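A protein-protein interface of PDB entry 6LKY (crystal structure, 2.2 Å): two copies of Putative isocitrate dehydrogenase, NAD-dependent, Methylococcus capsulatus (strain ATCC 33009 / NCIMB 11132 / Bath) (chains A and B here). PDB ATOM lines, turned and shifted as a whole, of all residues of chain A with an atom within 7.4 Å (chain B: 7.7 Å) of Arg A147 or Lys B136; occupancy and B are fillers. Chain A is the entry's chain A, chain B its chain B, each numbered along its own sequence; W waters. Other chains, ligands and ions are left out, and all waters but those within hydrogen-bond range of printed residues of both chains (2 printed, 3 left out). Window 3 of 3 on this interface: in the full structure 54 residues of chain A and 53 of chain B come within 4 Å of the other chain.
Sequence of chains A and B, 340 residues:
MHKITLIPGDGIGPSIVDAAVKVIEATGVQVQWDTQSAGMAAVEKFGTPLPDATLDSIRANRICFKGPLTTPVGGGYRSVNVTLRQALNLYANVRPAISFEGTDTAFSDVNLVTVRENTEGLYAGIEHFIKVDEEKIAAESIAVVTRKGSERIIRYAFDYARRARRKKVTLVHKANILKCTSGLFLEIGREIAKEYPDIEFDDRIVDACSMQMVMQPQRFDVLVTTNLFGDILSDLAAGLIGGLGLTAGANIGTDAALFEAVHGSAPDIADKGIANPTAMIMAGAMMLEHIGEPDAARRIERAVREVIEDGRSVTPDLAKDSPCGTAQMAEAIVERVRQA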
ATOM      1  N   GLU A 120     -36.119  -6.854   9.554  1.00  0.00           N
ATOM      2  CA  GLU A 120     -34.711  -6.458   9.426  1.00  0.00           C
ATOM      3  C   GLU A 120     -34.537  -5.309   8.423  1.00  0.00           C
ATOM      4  O   GLU A 120     -35.311  -4.341   8.454  1.00  0.00           O
ATOM      5  CB  GLU A 120     -33.853  -7.684   9.059  1.00  0.00           C
ATOM      6  CG  GLU A 120     -34.385  -8.511   7.871  1.00  0.00           C
ATOM      7  CD  GLU A 120     -33.539  -9.753   7.546  1.00  0.00           C
ATOM      8  OE1 GLU A 120     -32.982 -10.368   8.486  1.00  0.00           O
ATOM      9  OE2 GLU A 120     -33.452 -10.135   6.348  1.00  0.00           O
ATOM     10  N   VAL A 145     -29.597  -7.618   5.917  1.00  0.00           N
ATOM     11  CA  VAL A 145     -30.350  -8.632   5.192  1.00  0.00           C
ATOM     12  C   VAL A 145     -29.708  -9.979   5.482  1.00  0.00           C
ATOM     13  O   VAL A 145     -28.505 -10.151   5.252  1.00  0.00           O
ATOM     14  CB  VAL A 145     -30.360  -8.350   3.679  1.00  0.00           C
ATOM     15  CG1 VAL A 145     -30.938  -9.538   2.912  1.00  0.00           C
ATOM     16  CG2 VAL A 145     -31.134  -7.072   3.385  1.00  0.00           C
ATOM     17  N   THR A 146     -30.508 -10.927   5.973  1.00  0.00           N
ATOM     18  CA  THR A 146     -30.087 -12.306   6.194  1.00  0.00           C
ATOM     19  C   THR A 146     -30.689 -13.201   5.119  1.00  0.00           C
ATOM     20  O   THR A 146     -31.748 -12.898   4.554  1.00  0.00           O
ATOM     21  CB  THR A 146     -30.521 -12.851   7.567  1.00  0.00           C
ATOM     22  OG1 THR A 146     -31.947 -12.822   7.653  1.00  0.00           O
ATOM     23  CG2 THR A 146     -29.915 -12.053   8.715  1.00  0.00           C
ATOM     24  N   ARG A 147     -29.990 -14.304   4.832  1.00  0.00           N
ATOM     25  CA  ARG A 147     -30.536 -15.314   3.925  1.00  0.00           C
ATOM     26  C   ARG A 147     -31.895 -15.824   4.405  1.00  0.00           C
ATOM     27  O   ARG A 147     -32.840 -15.940   3.614  1.00  0.00           O
ATOM     28  CB  ARG A 147     -29.541 -16.471   3.761  1.00  0.00           C
ATOM     29  CG  ARG A 147     -30.028 -17.597   2.830  1.00  0.00           C
ATOM     30  CD  ARG A 147     -28.924 -18.648   2.555  1.00  0.00           C
ATOM     31  NE  ARG A 147     -27.758 -18.085   1.874  1.00  0.00           N
ATOM     32  CZ  ARG A 147     -27.718 -17.796   0.573  1.00  0.00           C
ATOM     33  NH1 ARG A 147     -28.773 -18.025  -0.197  1.00  0.00           N
ATOM     34  NH2 ARG A 147     -26.620 -17.282   0.033  1.00  0.00           N
ATOM     35  N   LYS A 148     -32.036 -16.108   5.702  1.00  0.00           N
ATOM     36  CA  LYS A 148     -33.268 -16.786   6.088  1.00  0.00           C
ATOM     37  C   LYS A 148     -34.434 -15.807   6.188  1.00  0.00           C
ATOM     38  O   LYS A 148     -35.566 -16.172   5.839  1.00  0.00           O
ATOM     39  CB  LYS A 148     -33.100 -17.549   7.411  1.00  0.00           C
ATOM     40  CG  LYS A 148     -31.836 -18.409   7.538  1.00  0.00           C
ATOM     41  CD  LYS A 148     -31.979 -19.801   6.897  1.00  0.00           C
ATOM     42  CE  LYS A 148     -31.627 -19.788   5.392  1.00  0.00           C
ATOM     43  NZ  LYS A 148     -31.442 -21.163   4.807  1.00  0.00           N
ATOM     44  N   GLY A 149     -34.169 -14.546   6.564  1.00  0.00           N
ATOM     45  CA  GLY A 149     -35.212 -13.527   6.508  1.00  0.00           C
ATOM     46  C   GLY A 149     -35.748 -13.311   5.106  1.00  0.00           C
ATOM     47  O   GLY A 149     -36.969 -13.230   4.895  1.00  0.00           O
ATOM     48  N   SER A 150     -34.845 -13.256   4.123  1.00  0.00           N
ATOM     49  CA  SER A 150     -35.265 -13.082   2.732  1.00  0.00           C
ATOM     50  C   SER A 150     -36.055 -14.286   2.237  1.00  0.00           C
ATOM     51  O   SER A 150     -37.091 -14.136   1.575  1.00  0.00           O
ATOM     52  CB  SER A 150     -34.043 -12.848   1.844  1.00  0.00           C
ATOM     53  OG  SER A 150     -33.226 -11.844   2.389  1.00  0.00           O
ATOM     54  N   GLU A 151     -35.545 -15.489   2.507  1.00  0.00           N
ATOM     55  CA  GLU A 151     -36.229 -16.710   2.098  1.00  0.00           C
ATOM     56  C   GLU A 151     -37.657 -16.739   2.614  1.00  0.00           C
ATOM     57  O   GLU A 151     -38.602 -17.023   1.864  1.00  0.00           O
ATOM     58  CB  GLU A 151     -35.467 -17.939   2.596  1.00  0.00           C
ATOM     59  CG  GLU A 151     -34.272 -18.310   1.741  1.00  0.00           C
ATOM     60  CD  GLU A 151     -33.410 -19.359   2.412  1.00  0.00           C
ATOM     61  OE1 GLU A 151     -33.839 -19.848   3.477  1.00  0.00           O
ATOM     62  OE2 GLU A 151     -32.311 -19.683   1.893  1.00  0.00           O
ATOM     63  N   ARG A 152     -37.836 -16.448   3.900  1.00  0.00           N
ATOM     64  CA  ARG A 152     -39.172 -16.607   4.450  1.00  0.00           C
ATOM     65  C   ARG A 152     -40.123 -15.532   3.929  1.00  0.00           C
ATOM     66  O   ARG A 152     -41.284 -15.840   3.623  1.00  0.00           O
ATOM     67  CB  ARG A 152     -39.122 -16.644   5.982  1.00  0.00           C
ATOM     68  CG  ARG A 152     -38.638 -15.376   6.682  1.00  0.00           C
ATOM     69  CD  ARG A 152     -38.656 -15.570   8.209  1.00  0.00           C
ATOM     70  NE  ARG A 152     -38.165 -14.391   8.919  1.00  0.00           N
ATOM     71  CZ  ARG A 152     -38.019 -14.325  10.240  1.00  0.00           C
ATOM     72  NH1 ARG A 152     -38.329 -15.369  10.997  1.00  0.00           N
ATOM     73  NH2 ARG A 152     -37.580 -13.206  10.807  1.00  0.00           N
ATOM     74  N   ILE A 153     -39.656 -14.280   3.750  1.00  0.00           N
ATOM     75  CA  ILE A 153     -40.597 -13.273   3.241  1.00  0.00           C
ATOM     76  C   ILE A 153     -40.951 -13.543   1.775  1.00  0.00           C
ATOM     77  O   ILE A 153     -42.108 -13.360   1.359  1.00  0.00           O
ATOM     78  CB  ILE A 153     -40.084 -11.827   3.459  1.00  0.00           C
ATOM     79  CG1 ILE A 153     -41.230 -10.827   3.235  1.00  0.00           C
ATOM     80  CG2 ILE A 153     -38.930 -11.453   2.524  1.00  0.00           C
ATOM     81  CD1 ILE A 153     -42.383 -10.973   4.237  1.00  0.00           C
ATOM     82  N   ILE A 154     -39.994 -14.019   0.973  1.00  0.00           N
ATOM     83  CA  ILE A 154     -40.310 -14.234  -0.439  1.00  0.00           C
ATOM     84  C   ILE A 154     -41.197 -15.471  -0.616  1.00  0.00           C
ATOM     85  O   ILE A 154     -42.147 -15.460  -1.420  1.00  0.00           O
ATOM     86  CB  ILE A 154     -39.022 -14.310  -1.280  1.00  0.00           C
ATOM     87  CG1 ILE A 154     -38.317 -12.938  -1.296  1.00  0.00           C
ATOM     88  CG2 ILE A 154     -39.350 -14.791  -2.721  1.00  0.00           C
ATOM     89  CD1 ILE A 154     -36.786 -13.004  -1.496  1.00  0.00           C
ATOM     90  N   ARG A 155     -40.925 -16.547   0.140  1.00  0.00           N
ATOM     91  CA  ARG A 155     -41.846 -17.678   0.120  1.00  0.00           C
ATOM     92  C   ARG A 155     -43.231 -17.264   0.602  1.00  0.00           C
ATOM     93  O   ARG A 155     -44.240 -17.713   0.044  1.00  0.00           O
ATOM     94  CB  ARG A 155     -41.317 -18.832   0.974  1.00  0.00           C
ATOM     95  CG  ARG A 155     -40.087 -19.506   0.408  1.00  0.00           C
ATOM     96  CD  ARG A 155     -39.975 -20.947   0.854  1.00  0.00           C
ATOM     97  NE  ARG A 155     -38.981 -21.652   0.054  1.00  0.00           N
ATOM     98  CZ  ARG A 155     -37.723 -21.823   0.438  1.00  0.00           C
ATOM     99  NH1 ARG A 155     -37.330 -21.365   1.621  1.00  0.00           N
ATOM    100  NH2 ARG A 155     -36.867 -22.468  -0.346  1.00  0.00           N
ATOM    101  N   LYS A 179     -25.653  -3.447  -3.634  1.00  0.00           N
ATOM    102  CA  LYS A 179     -25.282  -4.703  -4.287  1.00  0.00           C
ATOM    103  C   LYS A 179     -25.286  -5.882  -3.317  1.00  0.00           C
ATOM    104  O   LYS A 179     -25.577  -7.012  -3.723  1.00  0.00           O
ATOM    105  CB  LYS A 179     -23.912  -4.562  -4.960  1.00  0.00           C
ATOM    106  CG  LYS A 179     -23.908  -3.604  -6.167  1.00  0.00           C
ATOM    107  CD  LYS A 179     -22.550  -3.605  -6.876  1.00  0.00           C
ATOM    108  CE  LYS A 179     -22.478  -2.566  -7.999  1.00  0.00           C
ATOM    109  NZ  LYS A 179     -23.343  -2.902  -9.177  1.00  0.00           N
ATOM    110  N   CYS A 180     -24.982  -5.646  -2.041  1.00  0.00           N
ATOM    111  CA  CYS A 180     -24.906  -6.743  -1.085  1.00  0.00           C
ATOM    112  C   CYS A 180     -26.260  -7.084  -0.486  1.00  0.00           C
ATOM    113  O   CYS A 180     -26.665  -8.243  -0.521  1.00  0.00           O
ATOM    114  CB  CYS A 180     -23.901  -6.411   0.026  1.00  0.00           C
ATOM    115  SG  CYS A 180     -22.197  -6.379  -0.598  1.00  0.00           S
ATOM    116  N   GLY A 183     -29.017  -6.867  -3.362  1.00  0.00           N
ATOM    117  CA  GLY A 183     -28.568  -7.889  -4.302  1.00  0.00           C
ATOM    118  C   GLY A 183     -28.814  -9.307  -3.808  1.00  0.00           C
ATOM    119  O   GLY A 183     -29.232 -10.175  -4.578  1.00  0.00           O
ATOM    120  N   LEU A 184     -28.524  -9.569  -2.527  1.00  0.00           N
ATOM    121  CA  LEU A 184     -28.809 -10.886  -1.956  1.00  0.00           C
ATOM    122  C   LEU A 184     -30.313 -11.148  -1.916  1.00  0.00           C
ATOM    123  O   LEU A 184     -30.774 -12.250  -2.245  1.00  0.00           O
ATOM    124  CB  LEU A 184     -28.203 -10.990  -0.557  1.00  0.00           C
ATOM    125  CG  LEU A 184     -28.378 -12.302   0.215  1.00  0.00           C
ATOM    126  CD1 LEU A 184     -27.689 -13.457  -0.515  1.00  0.00           C
ATOM    127  CD2 LEU A 184     -27.852 -12.169   1.641  1.00  0.00           C
ATOM    128  N   GLU A 187     -31.291 -12.039  -5.517  1.00  0.00           N
ATOM    129  CA  GLU A 187     -30.779 -13.351  -5.909  1.00  0.00           C
ATOM    130  C   GLU A 187     -31.590 -14.474  -5.272  1.00  0.00           C
ATOM    131  O   GLU A 187     -31.965 -15.454  -5.937  1.00  0.00           O
ATOM    132  CB  GLU A 187     -29.308 -13.455  -5.514  1.00  0.00           C
ATOM    133  CG  GLU A 187     -28.686 -14.821  -5.735  1.00  0.00           C
ATOM    134  CD  GLU A 187     -27.379 -14.958  -4.987  1.00  0.00           C
ATOM    135  OE1 GLU A 187     -26.471 -14.139  -5.252  1.00  0.00           O
ATOM    136  OE2 GLU A 187     -27.267 -15.866  -4.128  1.00  0.00           O
ATOM    137  N   ILE A 188     -31.885 -14.338  -3.976  1.00  0.00           N
ATOM    138  CA  ILE A 188     -32.715 -15.330  -3.307  1.00  0.00           C
ATOM    139  C   ILE A 188     -34.109 -15.379  -3.929  1.00  0.00           C
ATOM    140  O   ILE A 188     -34.676 -16.464  -4.129  1.00  0.00           O
ATOM    141  CB  ILE A 188     -32.759 -15.045  -1.799  1.00  0.00           C
ATOM    142  CG1 ILE A 188     -31.401 -15.395  -1.180  1.00  0.00           C
ATOM    143  CG2 ILE A 188     -33.893 -15.803  -1.171  1.00  0.00           C
ATOM    144  CD1 ILE A 188     -31.181 -14.857   0.225  1.00  0.00           C
ATOM    145  N   GLU A 191     -34.036 -17.354  -7.093  1.00  0.00           N
ATOM    146  CA  GLU A 191     -33.944 -18.791  -6.850  1.00  0.00           C
ATOM    147  C   GLU A 191     -35.292 -19.356  -6.414  1.00  0.00           C
ATOM    148  O   GLU A 191     -35.752 -20.371  -6.944  1.00  0.00           O
ATOM    149  CB  GLU A 191     -32.852 -19.088  -5.820  1.00  0.00           C
ATOM    150  CG  GLU A 191     -31.456 -19.034  -6.426  1.00  0.00           C
ATOM    151  CD  GLU A 191     -30.338 -18.904  -5.392  1.00  0.00           C
ATOM    152  OE1 GLU A 191     -29.182 -18.672  -5.815  1.00  0.00           O
ATOM    153  OE2 GLU A 191     -30.602 -19.022  -4.171  1.00  0.00           O
ATOM    154  N   ILE A 192     -35.971 -18.670  -5.491  1.00  0.00           N
ATOM    155  CA  ILE A 192     -37.229 -19.188  -4.961  1.00  0.00           C
ATOM    156  C   ILE A 192     -38.332 -19.166  -6.019  1.00  0.00           C
ATOM    157  O   ILE A 192     -39.234 -20.016  -6.001  1.00  0.00           O
ATOM    158  CB  ILE A 192     -37.617 -18.391  -3.701  1.00  0.00           C
ATOM    159  CG1 ILE A 192     -36.751 -18.836  -2.513  1.00  0.00           C
ATOM    160  CG2 ILE A 192     -39.130 -18.501  -3.397  1.00  0.00           C
ATOM    161  CD1 ILE A 192     -36.938 -18.008  -1.260  1.00  0.00           C
ATOM    162  N   GLY B  74     -26.792  -6.404  -8.516  1.00  0.00           N
ATOM    163  CA  GLY B  74     -26.354  -7.518  -7.693  1.00  0.00           C
ATOM    164  C   GLY B  74     -24.868  -7.767  -7.705  1.00  0.00           C
ATOM    165  O   GLY B  74     -24.381  -8.606  -6.935  1.00  0.00           O
ATOM    166  N   PHE B 129     -20.687  -8.623   2.578  1.00  0.00           N
ATOM    167  CA  PHE B 129     -21.325  -9.868   2.960  1.00  0.00           C
ATOM    168  C   PHE B 129     -20.741 -10.345   4.283  1.00  0.00           C
ATOM    169  O   PHE B 129     -19.593 -10.054   4.613  1.00  0.00           O
ATOM    170  CB  PHE B 129     -21.113 -10.931   1.880  1.00  0.00           C
ATOM    171  CG  PHE B 129     -21.714 -10.575   0.546  1.00  0.00           C
ATOM    172  CD1 PHE B 129     -23.095 -10.670   0.342  1.00  0.00           C
ATOM    173  CD2 PHE B 129     -20.902 -10.169  -0.516  1.00  0.00           C
ATOM    174  CE1 PHE B 129     -23.658 -10.353  -0.893  1.00  0.00           C
ATOM    175  CE2 PHE B 129     -21.455  -9.857  -1.753  1.00  0.00           C
ATOM    176  CZ  PHE B 129     -22.842  -9.946  -1.941  1.00  0.00           C
ATOM    177  N   ILE B 130     -21.549 -11.058   5.049  1.00  0.00           N
ATOM    178  CA  ILE B 130     -21.068 -11.870   6.152  1.00  0.00           C
ATOM    179  C   ILE B 130     -21.118 -13.308   5.672  1.00  0.00           C
ATOM    180  O   ILE B 130     -22.202 -13.822   5.329  1.00  0.00           O
ATOM    181  CB  ILE B 130     -21.904 -11.686   7.431  1.00  0.00           C
ATOM    182  CG1 ILE B 130     -21.690 -10.289   8.023  1.00  0.00           C
ATOM    183  CG2 ILE B 130     -21.513 -12.752   8.461  1.00  0.00           C
ATOM    184  CD1 ILE B 130     -22.803  -9.332   7.720  1.00  0.00           C
ATOM    185  N   LYS B 131     -19.933 -13.924   5.638  1.00  0.00           N
ATOM    186  CA  LYS B 131     -19.688 -15.224   5.048  1.00  0.00           C
ATOM    187  C   LYS B 131     -18.975 -16.129   6.034  1.00  0.00           C
ATOM    188  O   LYS B 131     -18.216 -15.673   6.897  1.00  0.00           O
ATOM    189  CB  LYS B 131     -18.787 -15.149   3.807  1.00  0.00           C
ATOM    190  CG  LYS B 131     -19.263 -14.317   2.646  1.00  0.00           C
ATOM    191  CD  LYS B 131     -18.261 -14.430   1.496  1.00  0.00           C
ATOM    192  CE  LYS B 131     -18.671 -13.576   0.307  1.00  0.00           C
ATOM    193  NZ  LYS B 131     -17.825 -13.844  -0.893  1.00  0.00           N
ATOM    194  N   VAL B 132     -19.221 -17.425   5.898  1.00  0.00           N
ATOM    195  CA  VAL B 132     -18.349 -18.449   6.456  1.00  0.00           C
ATOM    196  C   VAL B 132     -17.740 -19.167   5.263  1.00  0.00           C
ATOM    197  O   VAL B 132     -18.446 -19.851   4.510  1.00  0.00           O
ATOM    198  CB  VAL B 132     -19.089 -19.415   7.388  1.00  0.00           C
ATOM    199  CG1 VAL B 132     -18.089 -20.348   8.056  1.00  0.00           C
ATOM    200  CG2 VAL B 132     -19.874 -18.635   8.441  1.00  0.00           C
ATOM    201  N   ASP B 133     -16.437 -18.976   5.076  1.00  0.00           N
ATOM    202  CA  ASP B 133     -15.750 -19.386   3.860  1.00  0.00           C
ATOM    203  C   ASP B 133     -16.461 -18.729   2.680  1.00  0.00           C
ATOM    204  O   ASP B 133     -16.470 -17.501   2.565  1.00  0.00           O
ATOM    205  CB  ASP B 133     -15.689 -20.911   3.746  1.00  0.00           C
ATOM    206  CG  ASP B 133     -14.847 -21.541   4.855  1.00  0.00           C
ATOM    207  OD1 ASP B 133     -13.958 -20.845   5.413  1.00  0.00           O
ATOM    208  OD2 ASP B 133     -15.087 -22.723   5.180  1.00  0.00           O
ATOM    209  N   GLU B 134     -17.081 -19.514   1.814  1.00  0.00           N
ATOM    210  CA  GLU B 134     -17.677 -18.968   0.609  1.00  0.00           C
ATOM    211  C   GLU B 134     -19.201 -18.876   0.681  1.00  0.00           C
ATOM    212  O   GLU B 134     -19.833 -18.371  -0.253  1.00  0.00           O
ATOM    213  CB  GLU B 134     -17.211 -19.804  -0.592  1.00  0.00           C
ATOM    214  CG  GLU B 134     -15.685 -19.646  -0.884  1.00  0.00           C
ATOM    215  CD  GLU B 134     -14.769 -20.332   0.156  1.00  0.00           C
ATOM    216  OE1 GLU B 134     -15.000 -21.535   0.459  1.00  0.00           O
ATOM    217  OE2 GLU B 134     -13.822 -19.667   0.670  1.00  0.00           O
ATOM    218  N   GLU B 135     -19.803 -19.303   1.781  1.00  0.00           N
ATOM    219  CA  GLU B 135     -21.247 -19.237   1.949  1.00  0.00           C
ATOM    220  C   GLU B 135     -21.660 -17.899   2.567  1.00  0.00           C
ATOM    221  O   GLU B 135     -21.163 -17.516   3.635  1.00  0.00           O
ATOM    222  CB  GLU B 135     -21.719 -20.410   2.811  1.00  0.00           C
ATOM    223  CG  GLU B 135     -23.218 -20.478   2.980  1.00  0.00           C
ATOM    224  CD  GLU B 135     -23.632 -21.242   4.222  1.00  0.00           C
ATOM    225  OE1 GLU B 135     -24.844 -21.491   4.380  1.00  0.00           O
ATOM    226  OE2 GLU B 135     -22.750 -21.604   5.034  1.00  0.00           O
ATOM    227  N   LYS B 136     -22.583 -17.205   1.895  1.00  0.00           N
ATOM    228  CA  LYS B 136     -23.114 -15.925   2.360  1.00  0.00           C
ATOM    229  C   LYS B 136     -24.262 -16.170   3.333  1.00  0.00           C
ATOM    230  O   LYS B 136     -25.298 -16.721   2.946  1.00  0.00           O
ATOM    231  CB  LYS B 136     -23.628 -15.087   1.185  1.00  0.00           C
ATOM    232  CG  LYS B 136     -22.578 -14.591   0.203  1.00  0.00           C
ATOM    233  CD  LYS B 136     -23.270 -14.090  -1.060  1.00  0.00           C
ATOM    234  CE  LYS B 136     -22.285 -13.725  -2.159  1.00  0.00           C
ATOM    235  NZ  LYS B 136     -23.038 -13.388  -3.402  1.00  0.00           N
ATOM    236  N   ILE B 137     -24.100 -15.767   4.591  1.00  0.00           N
ATOM    237  CA  ILE B 137     -25.198 -15.917   5.536  1.00  0.00           C
ATOM    238  C   ILE B 137     -25.956 -14.608   5.734  1.00  0.00           C
ATOM    239  O   ILE B 137     -27.136 -14.645   6.128  1.00  0.00           O
ATOM    240  CB  ILE B 137     -24.719 -16.482   6.892  1.00  0.00           C
ATOM    241  CG1 ILE B 137     -23.827 -15.488   7.618  1.00  0.00           C
ATOM    242  CG2 ILE B 137     -23.984 -17.812   6.693  1.00  0.00           C
ATOM    243  CD1 ILE B 137     -23.501 -15.909   9.026  1.00  0.00           C
ATOM    244  N   ALA B 138     -25.333 -13.464   5.455  1.00  0.00           N
ATOM    245  CA  ALA B 138     -26.049 -12.203   5.604  1.00  0.00           C
ATOM    246  C   ALA B 138     -25.314 -11.137   4.814  1.00  0.00           C
ATOM    247  O   ALA B 138     -24.241 -11.378   4.276  1.00  0.00           O
ATOM    248  CB  ALA B 138     -26.180 -11.779   7.074  1.00  0.00           C
ATOM    249  N   ALA B 139     -25.904  -9.946   4.773  1.00  0.00           N
ATOM    250  CA  ALA B 139     -25.319  -8.807   4.093  1.00  0.00           C
ATOM    251  C   ALA B 139     -25.642  -7.540   4.871  1.00  0.00           C
ATOM    252  O   ALA B 139     -26.676  -7.445   5.540  1.00  0.00           O
ATOM    253  CB  ALA B 139     -25.849  -8.689   2.663  1.00  0.00           C
HETATM  254  O   HOH W   1     -29.276 -16.225   7.388  1.00  0.00           O
HETATM  255  O   HOH W   2     -23.627 -18.088  -0.286  1.00  0.00           O
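The backbone carbonyl oxygen of Val A145 sits at hydrogen-bond distance from the backbone NH of Ala B139 (2.7 Å). The guanidinium group of Arg A147 is in hydrogen-bond range of the backbone carbonyl oxygen of Lys B136, 3.0 Å away. The backbone carbonyl oxygen of Ile B137 is in hydrogen-bond range of the backbone NH of Arg A147 (3.2 Å). OE1 of Glu A187 lies within salt-bridge range of NZ of Lys B136, at 3.97 Å.
OG1 of Thr A146 is in hydrogen-bond range of OE1 of Glu A120, 2.8 Å away. The backbone NH of Gly A149 lies within hydrogen-bond range of the side-chain hydroxyl of Thr A146 (3.0 Å). The backbone carbonyl oxygen of Thr A146 is in hydrogen-bond range of the side-chain hydroxyl of Ser A150 (2.8 Å). O of Ile B130 sits at hydrogen-bond distance from N of Ile B137, at 2.8 Å. O of Ala B138 is in hydrogen-bond range of N of Ile B130 (2.8 Å).
Ala B138 touches Val A145. CA of Thr A146 touches O of Ile B137, at 3.8 Å. Lys A179 touches Gly B74. O of Cys A180 touches CE1 of Phe B129 (3.7 Å). Cys A180 touches Ala B139.
Of chain A, only Arg A147 and Glu A187 come within 4 Å of Lys B136. Of the printed residues of chain A, Phe B129 touches Cys A180 (3.7 Å). Of the printed residues of chain A, Ala B139 touches Val A145 (2.7 Å) and Cys A180 (3.3 Å). The nearest residue of chain B that does not touch Arg A147 is Ala B138 (4.5 Å).
Of the 12 printed residues of chain B, 6 touch a printed residue of chain A. Printed residues of chain B that touch a printed residue of chain A: Gly B74, Phe B129, Lys B136, Ile B137, Ala B138 and Ala B139. Along chain B the printed residues that touch a printed residue of chain A span positions 74 to 139.
No position is printed for both chains.
Water W2 lies within hydrogen-bond range of N of Lys B136 and NH2 of Arg A147. Water W1 lies within hydrogen-bond range of O of Ile B137, N of Lys A148 and N of Arg A147.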
